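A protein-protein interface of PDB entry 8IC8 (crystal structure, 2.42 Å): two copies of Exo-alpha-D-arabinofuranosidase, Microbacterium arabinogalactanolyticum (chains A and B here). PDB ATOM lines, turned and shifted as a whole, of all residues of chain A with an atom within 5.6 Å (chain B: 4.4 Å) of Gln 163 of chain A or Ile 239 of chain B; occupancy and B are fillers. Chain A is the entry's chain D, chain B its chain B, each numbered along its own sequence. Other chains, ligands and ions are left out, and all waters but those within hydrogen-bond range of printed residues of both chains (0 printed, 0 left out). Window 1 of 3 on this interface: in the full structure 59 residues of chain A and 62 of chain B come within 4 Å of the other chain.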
ATOM      1  N   THR A  15     -30.989 -23.130   8.023  1.00  0.00           N
ATOM      2  CA  THR A  15     -30.275 -23.998   7.089  1.00  0.00           C
ATOM      3  C   THR A  15     -28.925 -24.367   7.679  1.00  0.00           C
ATOM      4  O   THR A  15     -28.145 -23.480   8.048  1.00  0.00           O
ATOM      5  CB  THR A  15     -30.054 -23.337   5.721  1.00  0.00           C
ATOM      6  OG1 THR A  15     -31.309 -23.017   5.132  1.00  0.00           O
ATOM      7  CG2 THR A  15     -29.317 -24.274   4.785  1.00  0.00           C
ATOM      8  N   ARG A  16     -28.655 -25.671   7.756  1.00  0.00           N
ATOM      9  CA  ARG A  16     -27.358 -26.217   8.117  1.00  0.00           C
ATOM     10  C   ARG A  16     -26.860 -27.139   7.002  1.00  0.00           C
ATOM     11  O   ARG A  16     -27.630 -27.595   6.144  1.00  0.00           O
ATOM     12  CB  ARG A  16     -27.435 -26.981   9.444  1.00  0.00           C
ATOM     13  CG  ARG A  16     -27.996 -26.148  10.593  1.00  0.00           C
ATOM     14  CD  ARG A  16     -27.015 -25.056  11.013  1.00  0.00           C
ATOM     15  NE  ARG A  16     -27.568 -24.134  12.000  1.00  0.00           N
ATOM     16  CZ  ARG A  16     -27.892 -22.862  11.760  1.00  0.00           C
ATOM     17  NH1 ARG A  16     -27.748 -22.337  10.545  1.00  0.00           N
ATOM     18  NH2 ARG A  16     -28.370 -22.110  12.745  1.00  0.00           N
ATOM     19  N   SER A  17     -25.555 -27.408   7.015  1.00  0.00           N
ATOM     20  CA  SER A  17     -24.924 -28.192   5.959  1.00  0.00           C
ATOM     21  C   SER A  17     -23.779 -28.986   6.557  1.00  0.00           C
ATOM     22  O   SER A  17     -22.846 -28.402   7.110  1.00  0.00           O
ATOM     23  CB  SER A  17     -24.417 -27.293   4.834  1.00  0.00           C
ATOM     24  OG  SER A  17     -24.181 -28.058   3.664  1.00  0.00           O
ATOM     25  N   ILE A  18     -23.855 -30.303   6.463  1.00  0.00           N
ATOM     26  CA  ILE A  18     -22.812 -31.177   6.981  1.00  0.00           C
ATOM     27  C   ILE A  18     -21.842 -31.497   5.852  1.00  0.00           C
ATOM     28  O   ILE A  18     -22.261 -31.873   4.747  1.00  0.00           O
ATOM     29  CB  ILE A  18     -23.421 -32.457   7.577  1.00  0.00           C
ATOM     30  CG1 ILE A  18     -23.994 -32.169   8.966  1.00  0.00           C
ATOM     31  CG2 ILE A  18     -22.395 -33.594   7.623  1.00  0.00           C
ATOM     32  CD1 ILE A  18     -24.912 -33.259   9.476  1.00  0.00           C
ATOM     33  N   SER A  19     -20.550 -31.359   6.121  1.00  0.00           N
ATOM     34  CA  SER A  19     -19.531 -31.660   5.122  1.00  0.00           C
ATOM     35  C   SER A  19     -18.275 -32.079   5.860  1.00  0.00           C
ATOM     36  O   SER A  19     -18.215 -31.994   7.092  1.00  0.00           O
ATOM     37  CB  SER A  19     -19.261 -30.449   4.214  1.00  0.00           C
ATOM     38  OG  SER A  19     -18.393 -29.514   4.834  1.00  0.00           O
ATOM     39  N   PRO A  20     -17.254 -32.555   5.143  1.00  0.00           N
ATOM     40  CA  PRO A  20     -15.980 -32.849   5.825  1.00  0.00           C
ATOM     41  C   PRO A  20     -15.351 -31.632   6.490  1.00  0.00           C
ATOM     42  O   PRO A  20     -14.543 -31.804   7.408  1.00  0.00           O
ATOM     43  CB  PRO A  20     -15.096 -33.407   4.694  1.00  0.00           C
ATOM     44  CG  PRO A  20     -16.091 -33.985   3.720  1.00  0.00           C
ATOM     45  CD  PRO A  20     -17.232 -33.017   3.739  1.00  0.00           C
ATOM     46  N   ASN A  22     -17.263 -29.452   8.074  1.00  0.00           N
ATOM     47  CA  ASN A  22     -18.152 -29.157   9.210  1.00  0.00           C
ATOM     48  C   ASN A  22     -18.905 -30.458   9.538  1.00  0.00           C
ATOM     49  O   ASN A  22     -20.088 -30.630   9.209  1.00  0.00           O
ATOM     50  CB  ASN A  22     -19.101 -27.991   8.915  1.00  0.00           C
ATOM     51  CG  ASN A  22     -19.806 -27.471  10.173  1.00  0.00           C
ATOM     52  OD1 ASN A  22     -19.618 -28.003  11.266  1.00  0.00           O
ATOM     53  ND2 ASN A  22     -20.626 -26.436  10.015  1.00  0.00           N
ATOM     54  N   HIS A  76     -30.826 -30.922   0.166  1.00  0.00           N
ATOM     55  CA  HIS A  76     -29.875 -31.182  -0.910  1.00  0.00           C
ATOM     56  C   HIS A  76     -28.715 -32.037  -0.410  1.00  0.00           C
ATOM     57  O   HIS A  76     -28.118 -31.747   0.634  1.00  0.00           O
ATOM     58  CB  HIS A  76     -29.339 -29.875  -1.520  1.00  0.00           C
ATOM     59  CG  HIS A  76     -28.392 -30.098  -2.660  1.00  0.00           C
ATOM     60  ND1 HIS A  76     -27.119 -29.570  -2.694  1.00  0.00           N
ATOM     61  CD2 HIS A  76     -28.520 -30.833  -3.791  1.00  0.00           C
ATOM     62  CE1 HIS A  76     -26.511 -29.950  -3.805  1.00  0.00           C
ATOM     63  NE2 HIS A  76     -27.341 -30.715  -4.490  1.00  0.00           N
ATOM     64  N   ILE A  77     -28.396 -33.080  -1.172  1.00  0.00           N
ATOM     65  CA  ILE A  77     -27.174 -33.857  -1.004  1.00  0.00           C
ATOM     66  C   ILE A  77     -26.352 -33.689  -2.270  1.00  0.00           C
ATOM     67  O   ILE A  77     -26.850 -33.935  -3.376  1.00  0.00           O
ATOM     68  CB  ILE A  77     -27.453 -35.354  -0.772  1.00  0.00           C
ATOM     69  CG1 ILE A  77     -28.185 -35.589   0.560  1.00  0.00           C
ATOM     70  CG2 ILE A  77     -26.138 -36.165  -0.884  1.00  0.00           C
ATOM     71  CD1 ILE A  77     -28.629 -37.035   0.775  1.00  0.00           C
ATOM     72  N   TRP A  78     -25.107 -33.267  -2.114  1.00  0.00           N
ATOM     73  CA  TRP A  78     -24.108 -33.386  -3.164  1.00  0.00           C
ATOM     74  C   TRP A  78     -23.041 -34.355  -2.677  1.00  0.00           C
ATOM     75  O   TRP A  78     -22.746 -34.423  -1.480  1.00  0.00           O
ATOM     76  CB  TRP A  78     -23.481 -32.019  -3.529  1.00  0.00           C
ATOM     77  CG  TRP A  78     -22.289 -32.154  -4.430  1.00  0.00           C
ATOM     78  CD1 TRP A  78     -22.292 -32.161  -5.789  1.00  0.00           C
ATOM     79  CD2 TRP A  78     -20.916 -32.323  -4.029  1.00  0.00           C
ATOM     80  NE1 TRP A  78     -21.009 -32.316  -6.264  1.00  0.00           N
ATOM     81  CE2 TRP A  78     -20.149 -32.426  -5.203  1.00  0.00           C
ATOM     82  CE3 TRP A  78     -20.268 -32.410  -2.790  1.00  0.00           C
ATOM     83  CZ2 TRP A  78     -18.765 -32.601  -5.177  1.00  0.00           C
ATOM     84  CZ3 TRP A  78     -18.894 -32.579  -2.765  1.00  0.00           C
ATOM     85  CH2 TRP A  78     -18.161 -32.672  -3.951  1.00  0.00           C
ATOM     86  N   ILE A  79     -22.460 -35.113  -3.597  1.00  0.00           N
ATOM     87  CA  ILE A  79     -21.472 -36.115  -3.205  1.00  0.00           C
ATOM     88  C   ILE A  79     -20.691 -36.514  -4.447  1.00  0.00           C
ATOM     89  O   ILE A  79     -21.248 -36.590  -5.541  1.00  0.00           O
ATOM     90  CB  ILE A  79     -22.151 -37.334  -2.521  1.00  0.00           C
ATOM     91  CG1 ILE A  79     -21.109 -38.332  -1.994  1.00  0.00           C
ATOM     92  CG2 ILE A  79     -23.124 -38.042  -3.495  1.00  0.00           C
ATOM     93  CD1 ILE A  79     -21.668 -39.281  -0.946  1.00  0.00           C
ATOM     94  N   TYR A 161     -16.194 -37.069  -1.175  1.00  0.00           N
ATOM     95  CA  TYR A 161     -16.515 -35.677  -0.873  1.00  0.00           C
ATOM     96  C   TYR A 161     -18.024 -35.564  -0.742  1.00  0.00           C
ATOM     97  O   TYR A 161     -18.761 -36.118  -1.567  1.00  0.00           O
ATOM     98  CB  TYR A 161     -16.070 -34.712  -1.981  1.00  0.00           C
ATOM     99  CG  TYR A 161     -14.593 -34.623  -2.290  1.00  0.00           C
ATOM    100  CD1 TYR A 161     -13.913 -35.670  -2.923  1.00  0.00           C
ATOM    101  CD2 TYR A 161     -13.886 -33.464  -2.000  1.00  0.00           C
ATOM    102  CE1 TYR A 161     -12.545 -35.571  -3.223  1.00  0.00           C
ATOM    103  CE2 TYR A 161     -12.536 -33.352  -2.300  1.00  0.00           C
ATOM    104  CZ  TYR A 161     -11.874 -34.408  -2.909  1.00  0.00           C
ATOM    105  OH  TYR A 161     -10.544 -34.267  -3.191  1.00  0.00           O
ATOM    106  N   TYR A 162     -18.503 -34.828   0.256  1.00  0.00           N
ATOM    107  CA  TYR A 162     -19.954 -34.747   0.375  1.00  0.00           C
ATOM    108  C   TYR A 162     -20.381 -33.415   0.989  1.00  0.00           C
ATOM    109  O   TYR A 162     -19.595 -32.698   1.608  1.00  0.00           O
ATOM    110  CB  TYR A 162     -20.503 -35.930   1.182  1.00  0.00           C
ATOM    111  CG  TYR A 162     -19.930 -36.001   2.572  1.00  0.00           C
ATOM    112  CD1 TYR A 162     -18.745 -36.689   2.826  1.00  0.00           C
ATOM    113  CD2 TYR A 162     -20.563 -35.360   3.639  1.00  0.00           C
ATOM    114  CE1 TYR A 162     -18.206 -36.742   4.115  1.00  0.00           C
ATOM    115  CE2 TYR A 162     -20.031 -35.412   4.930  1.00  0.00           C
ATOM    116  CZ  TYR A 162     -18.852 -36.103   5.157  1.00  0.00           C
ATOM    117  OH  TYR A 162     -18.326 -36.161   6.424  1.00  0.00           O
ATOM    118  N   GLN A 163     -21.649 -33.094   0.788  1.00  0.00           N
ATOM    119  CA  GLN A 163     -22.263 -31.891   1.332  1.00  0.00           C
ATOM    120  C   GLN A 163     -23.738 -32.219   1.490  1.00  0.00           C
ATOM    121  O   GLN A 163     -24.416 -32.506   0.496  1.00  0.00           O
ATOM    122  CB  GLN A 163     -22.060 -30.691   0.403  1.00  0.00           C
ATOM    123  CG  GLN A 163     -22.319 -29.347   1.052  1.00  0.00           C
ATOM    124  CD  GLN A 163     -21.079 -28.758   1.715  1.00  0.00           C
ATOM    125  OE1 GLN A 163     -19.961 -28.965   1.249  1.00  0.00           O
ATOM    126  NE2 GLN A 163     -21.274 -28.023   2.815  1.00  0.00           N
ATOM    127  N   VAL A 164     -24.212 -32.227   2.731  1.00  0.00           N
ATOM    128  CA  VAL A 164     -25.560 -32.656   3.074  1.00  0.00           C
ATOM    129  C   VAL A 164     -26.215 -31.453   3.732  1.00  0.00           C
ATOM    130  O   VAL A 164     -25.923 -31.117   4.889  1.00  0.00           O
ATOM    131  CB  VAL A 164     -25.578 -33.878   4.000  1.00  0.00           C
ATOM    132  CG1 VAL A 164     -27.015 -34.242   4.382  1.00  0.00           C
ATOM    133  CG2 VAL A 164     -24.855 -35.060   3.359  1.00  0.00           C
ATOM    134  N   THR A 165     -27.090 -30.792   2.995  1.00  0.00           N
ATOM    135  CA  THR A 165     -27.720 -29.560   3.438  1.00  0.00           C
ATOM    136  C   THR A 165     -29.138 -29.881   3.893  1.00  0.00           C
ATOM    137  O   THR A 165     -29.811 -30.735   3.305  1.00  0.00           O
ATOM    138  CB  THR A 165     -27.671 -28.549   2.289  1.00  0.00           C
ATOM    139  OG1 THR A 165     -26.295 -28.341   1.969  1.00  0.00           O
ATOM    140  CG2 THR A 165     -28.343 -27.210   2.617  1.00  0.00           C
ATOM    141  N   ILE B 226     -16.356 -22.414  -1.060  1.00  0.00           N
ATOM    142  CA  ILE B 226     -17.292 -21.367  -0.659  1.00  0.00           C
ATOM    143  C   ILE B 226     -17.551 -21.474   0.845  1.00  0.00           C
ATOM    144  O   ILE B 226     -17.510 -22.565   1.432  1.00  0.00           O
ATOM    145  CB  ILE B 226     -18.598 -21.475  -1.473  1.00  0.00           C
ATOM    146  CG1 ILE B 226     -19.367 -20.156  -1.462  1.00  0.00           C
ATOM    147  CG2 ILE B 226     -19.512 -22.594  -0.967  1.00  0.00           C
ATOM    148  CD1 ILE B 226     -20.402 -20.084  -2.583  1.00  0.00           C
ATOM    149  N   LYS B 227     -17.799 -20.335   1.489  1.00  0.00           N
ATOM    150  CA  LYS B 227     -18.048 -20.329   2.921  1.00  0.00           C
ATOM    151  C   LYS B 227     -19.161 -19.335   3.212  1.00  0.00           C
ATOM    152  O   LYS B 227     -19.097 -18.184   2.759  1.00  0.00           O
ATOM    153  CB  LYS B 227     -16.769 -19.979   3.699  1.00  0.00           C
ATOM    154  CG  LYS B 227     -15.709 -21.095   3.691  1.00  0.00           C
ATOM    155  CD  LYS B 227     -14.404 -20.659   4.344  1.00  0.00           C
ATOM    156  CE  LYS B 227     -13.400 -21.790   4.348  1.00  0.00           C
ATOM    157  NZ  LYS B 227     -12.021 -21.317   4.618  1.00  0.00           N
ATOM    158  N   PHE B 228     -20.185 -19.784   3.953  1.00  0.00           N
ATOM    159  CA  PHE B 228     -21.338 -18.958   4.300  1.00  0.00           C
ATOM    160  C   PHE B 228     -21.253 -18.622   5.783  1.00  0.00           C
ATOM    161  O   PHE B 228     -21.488 -19.487   6.635  1.00  0.00           O
ATOM    162  CB  PHE B 228     -22.654 -19.667   3.972  1.00  0.00           C
ATOM    163  CG  PHE B 228     -22.984 -19.698   2.495  1.00  0.00           C
ATOM    164  CD1 PHE B 228     -22.439 -20.673   1.671  1.00  0.00           C
ATOM    165  CD2 PHE B 228     -23.830 -18.749   1.937  1.00  0.00           C
ATOM    166  CE1 PHE B 228     -22.732 -20.706   0.321  1.00  0.00           C
ATOM    167  CE2 PHE B 228     -24.123 -18.770   0.584  1.00  0.00           C
ATOM    168  CZ  PHE B 228     -23.581 -19.754  -0.225  1.00  0.00           C
ATOM    169  N   PRO B 237     -17.244 -20.031   9.408  1.00  0.00           N
ATOM    170  CA  PRO B 237     -18.573 -20.105   8.780  1.00  0.00           C
ATOM    171  C   PRO B 237     -19.463 -21.232   9.306  1.00  0.00           C
ATOM    172  O   PRO B 237     -19.031 -22.188   9.956  1.00  0.00           O
ATOM    173  CB  PRO B 237     -18.223 -20.369   7.316  1.00  0.00           C
ATOM    174  CG  PRO B 237     -16.965 -21.212   7.430  1.00  0.00           C
ATOM    175  CD  PRO B 237     -16.181 -20.470   8.493  1.00  0.00           C
ATOM    176  N   THR B 238     -20.744 -21.116   8.963  1.00  0.00           N
ATOM    177  CA  THR B 238     -21.718 -22.148   9.287  1.00  0.00           C
ATOM    178  C   THR B 238     -21.782 -23.214   8.197  1.00  0.00           C
ATOM    179  O   THR B 238     -21.755 -24.405   8.501  1.00  0.00           O
ATOM    180  CB  THR B 238     -23.085 -21.501   9.527  1.00  0.00           C
ATOM    181  OG1 THR B 238     -23.010 -20.723  10.728  1.00  0.00           O
ATOM    182  CG2 THR B 238     -24.181 -22.558   9.679  1.00  0.00           C
ATOM    183  N   ILE B 239     -21.847 -22.812   6.927  1.00  0.00           N
ATOM    184  CA  ILE B 239     -21.728 -23.729   5.800  1.00  0.00           C
ATOM    185  C   ILE B 239     -20.369 -23.514   5.154  1.00  0.00           C
ATOM    186  O   ILE B 239     -20.000 -22.374   4.851  1.00  0.00           O
ATOM    187  CB  ILE B 239     -22.865 -23.543   4.778  1.00  0.00           C
ATOM    188  CG1 ILE B 239     -24.225 -23.831   5.427  1.00  0.00           C
ATOM    189  CG2 ILE B 239     -22.656 -24.470   3.580  1.00  0.00           C
ATOM    190  CD1 ILE B 239     -25.398 -23.340   4.618  1.00  0.00           C
ATOM    191  N   CYS B 240     -19.624 -24.605   4.956  1.00  0.00           N
ATOM    192  CA  CYS B 240     -18.299 -24.569   4.338  1.00  0.00           C
ATOM    193  C   CYS B 240     -18.221 -25.679   3.302  1.00  0.00           C
ATOM    194  O   CYS B 240     -18.291 -26.857   3.668  1.00  0.00           O
ATOM    195  CB  CYS B 240     -17.192 -24.745   5.387  1.00  0.00           C
ATOM    196  SG  CYS B 240     -15.494 -24.668   4.712  1.00  0.00           S
ATOM    197  N   GLY B 241     -18.071 -25.305   2.027  1.00  0.00           N
ATOM    198  CA  GLY B 241     -18.049 -26.240   0.913  1.00  0.00           C
ATOM    199  C   GLY B 241     -16.711 -26.960   0.768  1.00  0.00           C
ATOM    200  O   GLY B 241     -15.811 -26.835   1.596  1.00  0.00           O
ATOM    201  N   THR B 242     -16.585 -27.740  -0.315  1.00  0.00           N
ATOM    202  CA  THR B 242     -15.407 -28.584  -0.504  1.00  0.00           C
ATOM    203  C   THR B 242     -14.663 -28.346  -1.813  1.00  0.00           C
ATOM    204  O   THR B 242     -13.674 -29.038  -2.074  1.00  0.00           O
ATOM    205  CB  THR B 242     -15.767 -30.079  -0.429  1.00  0.00           C
ATOM    206  OG1 THR B 242     -16.584 -30.440  -1.544  1.00  0.00           O
ATOM    207  CG2 THR B 242     -16.496 -30.422   0.875  1.00  0.00           C
ATOM    208  N   ILE B 298     -30.459 -21.090   1.648  1.00  0.00           N
ATOM    209  CA  ILE B 298     -29.617 -20.925   2.825  1.00  0.00           C
ATOM    210  C   ILE B 298     -30.233 -19.809   3.666  1.00  0.00           C
ATOM    211  O   ILE B 298     -30.000 -18.615   3.426  1.00  0.00           O
ATOM    212  CB  ILE B 298     -28.157 -20.653   2.451  1.00  0.00           C
ATOM    213  CG1 ILE B 298     -27.565 -21.880   1.732  1.00  0.00           C
ATOM    214  CG2 ILE B 298     -27.349 -20.311   3.690  1.00  0.00           C
ATOM    215  CD1 ILE B 298     -26.156 -21.660   1.136  1.00  0.00           C
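No position is printed for both chains.
Of the 12 pairs that touch across the chains among the printed residues, none has its exchanged pair printed and touching as well.
Of the 16 printed residues of chain A, 9 touch a printed residue of chain B.
Printed residues of chain A that touch a printed residue of chain B: Thr 15, Arg 16, Ser 17, Ser 19, Pro 20, Asn 22, Trp 78, Tyr 162 and Gln 163.
Hydrophobic or aromatic side chains of chain A that line the printed part of chain B: Pro 20 and Trp 78.
Among the printed residues, 12 pairs touch across the chains.
The backbone NH (N) of Gly 241 of chain B sits at hydrogen-bond distance from the backbone carbonyl oxygen (O) of Ile 226 of chain B (2.9 Å).
O of Phe 228 of chain B lies within hydrogen-bond range of N of Thr 238 of chain B.
The side-chain hydroxyl (OG) of Ser 17 of chain A lies within hydrogen-bond range of the side-chain amide nitrogen (NE2) of Gln 163 of chain A (3.0 Å).
OG of Ser 17 of chain A lies within hydrogen-bond range of OG1 of Thr 165 of chain A (2.7 Å).
N of Asn 22 of chain A lies within hydrogen-bond range of OG of Ser 19 of chain A (3.4 Å).
N of Trp 78 of chain A lies within hydrogen-bond range of O of Gln 163 of chain A.
Of the printed residues of chain B, Thr 15 of chain A touches Ile 298 (3.5 Å).
Of the printed residues of chain B, Asn 22 of chain A touches Thr 238.
Ile 239 of chain B touches just these residues of chain A: Ser 17 (3.5 Å) and Gln 163 (3.9 Å).
Of the printed residues of chain A, Cys 240 of chain B touches Ser 19 (2.9 Å) and Gln 163 (3.3 Å).
Of the printed residues of chain A, Gly 241 of chain B touches Gln 163 (3.3 Å).
The nearest residue of chain A that does not touch Ile 239 of chain B is Thr 15 of chain A (4.03 Å).
The nearest printed residue of chain B that does not touch Trp 78 of chain A is Gly 241 of chain B (7.0 Å).
Thr 15 of chain A touches Ile 298 of chain B (OG1 to CA, 3.5 Å).
Thr 238 of chain B touches Arg 16 of chain A.
Ser 17 of chain A touches Ile 239 of chain B.
Pro 20 of chain A touches Thr 242 of chain B.
OG1 of Thr 242 of chain B touches CZ3 of Trp 78 of chain A, 3.4 Å away.
CG2 of Thr 242 of chain B touches O of Tyr 162 of chain A, at 3.9 Å.
Gln 163 of chain A touches Ile 239 of chain B (NE2 to CG2, 3.9 Å).
Gly 241 of chain B touches Gln 163 of chain A (CA to OE1, 3.3 Å).
OE1 of Gln 163 of chain A touches CG2 of Thr 242 of chain B, 3.8 Å away.
The backbone carbonyl oxygen (O) of Thr 238 of chain B is in hydrogen-bond range of the side-chain amide nitrogen (ND2) of Asn 22 of chain A (2.8 Å).
The backbone carbonyl oxygen (O) of Cys 240 of chain B is in hydrogen-bond range of the side-chain hydroxyl (OG) of Ser 19 of chain A.
The backbone carbonyl oxygen of Cys 240 of chain B sits at hydrogen-bond distance from the side-chain amide nitrogen of Gln 163 of chain A (3.3 Å).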
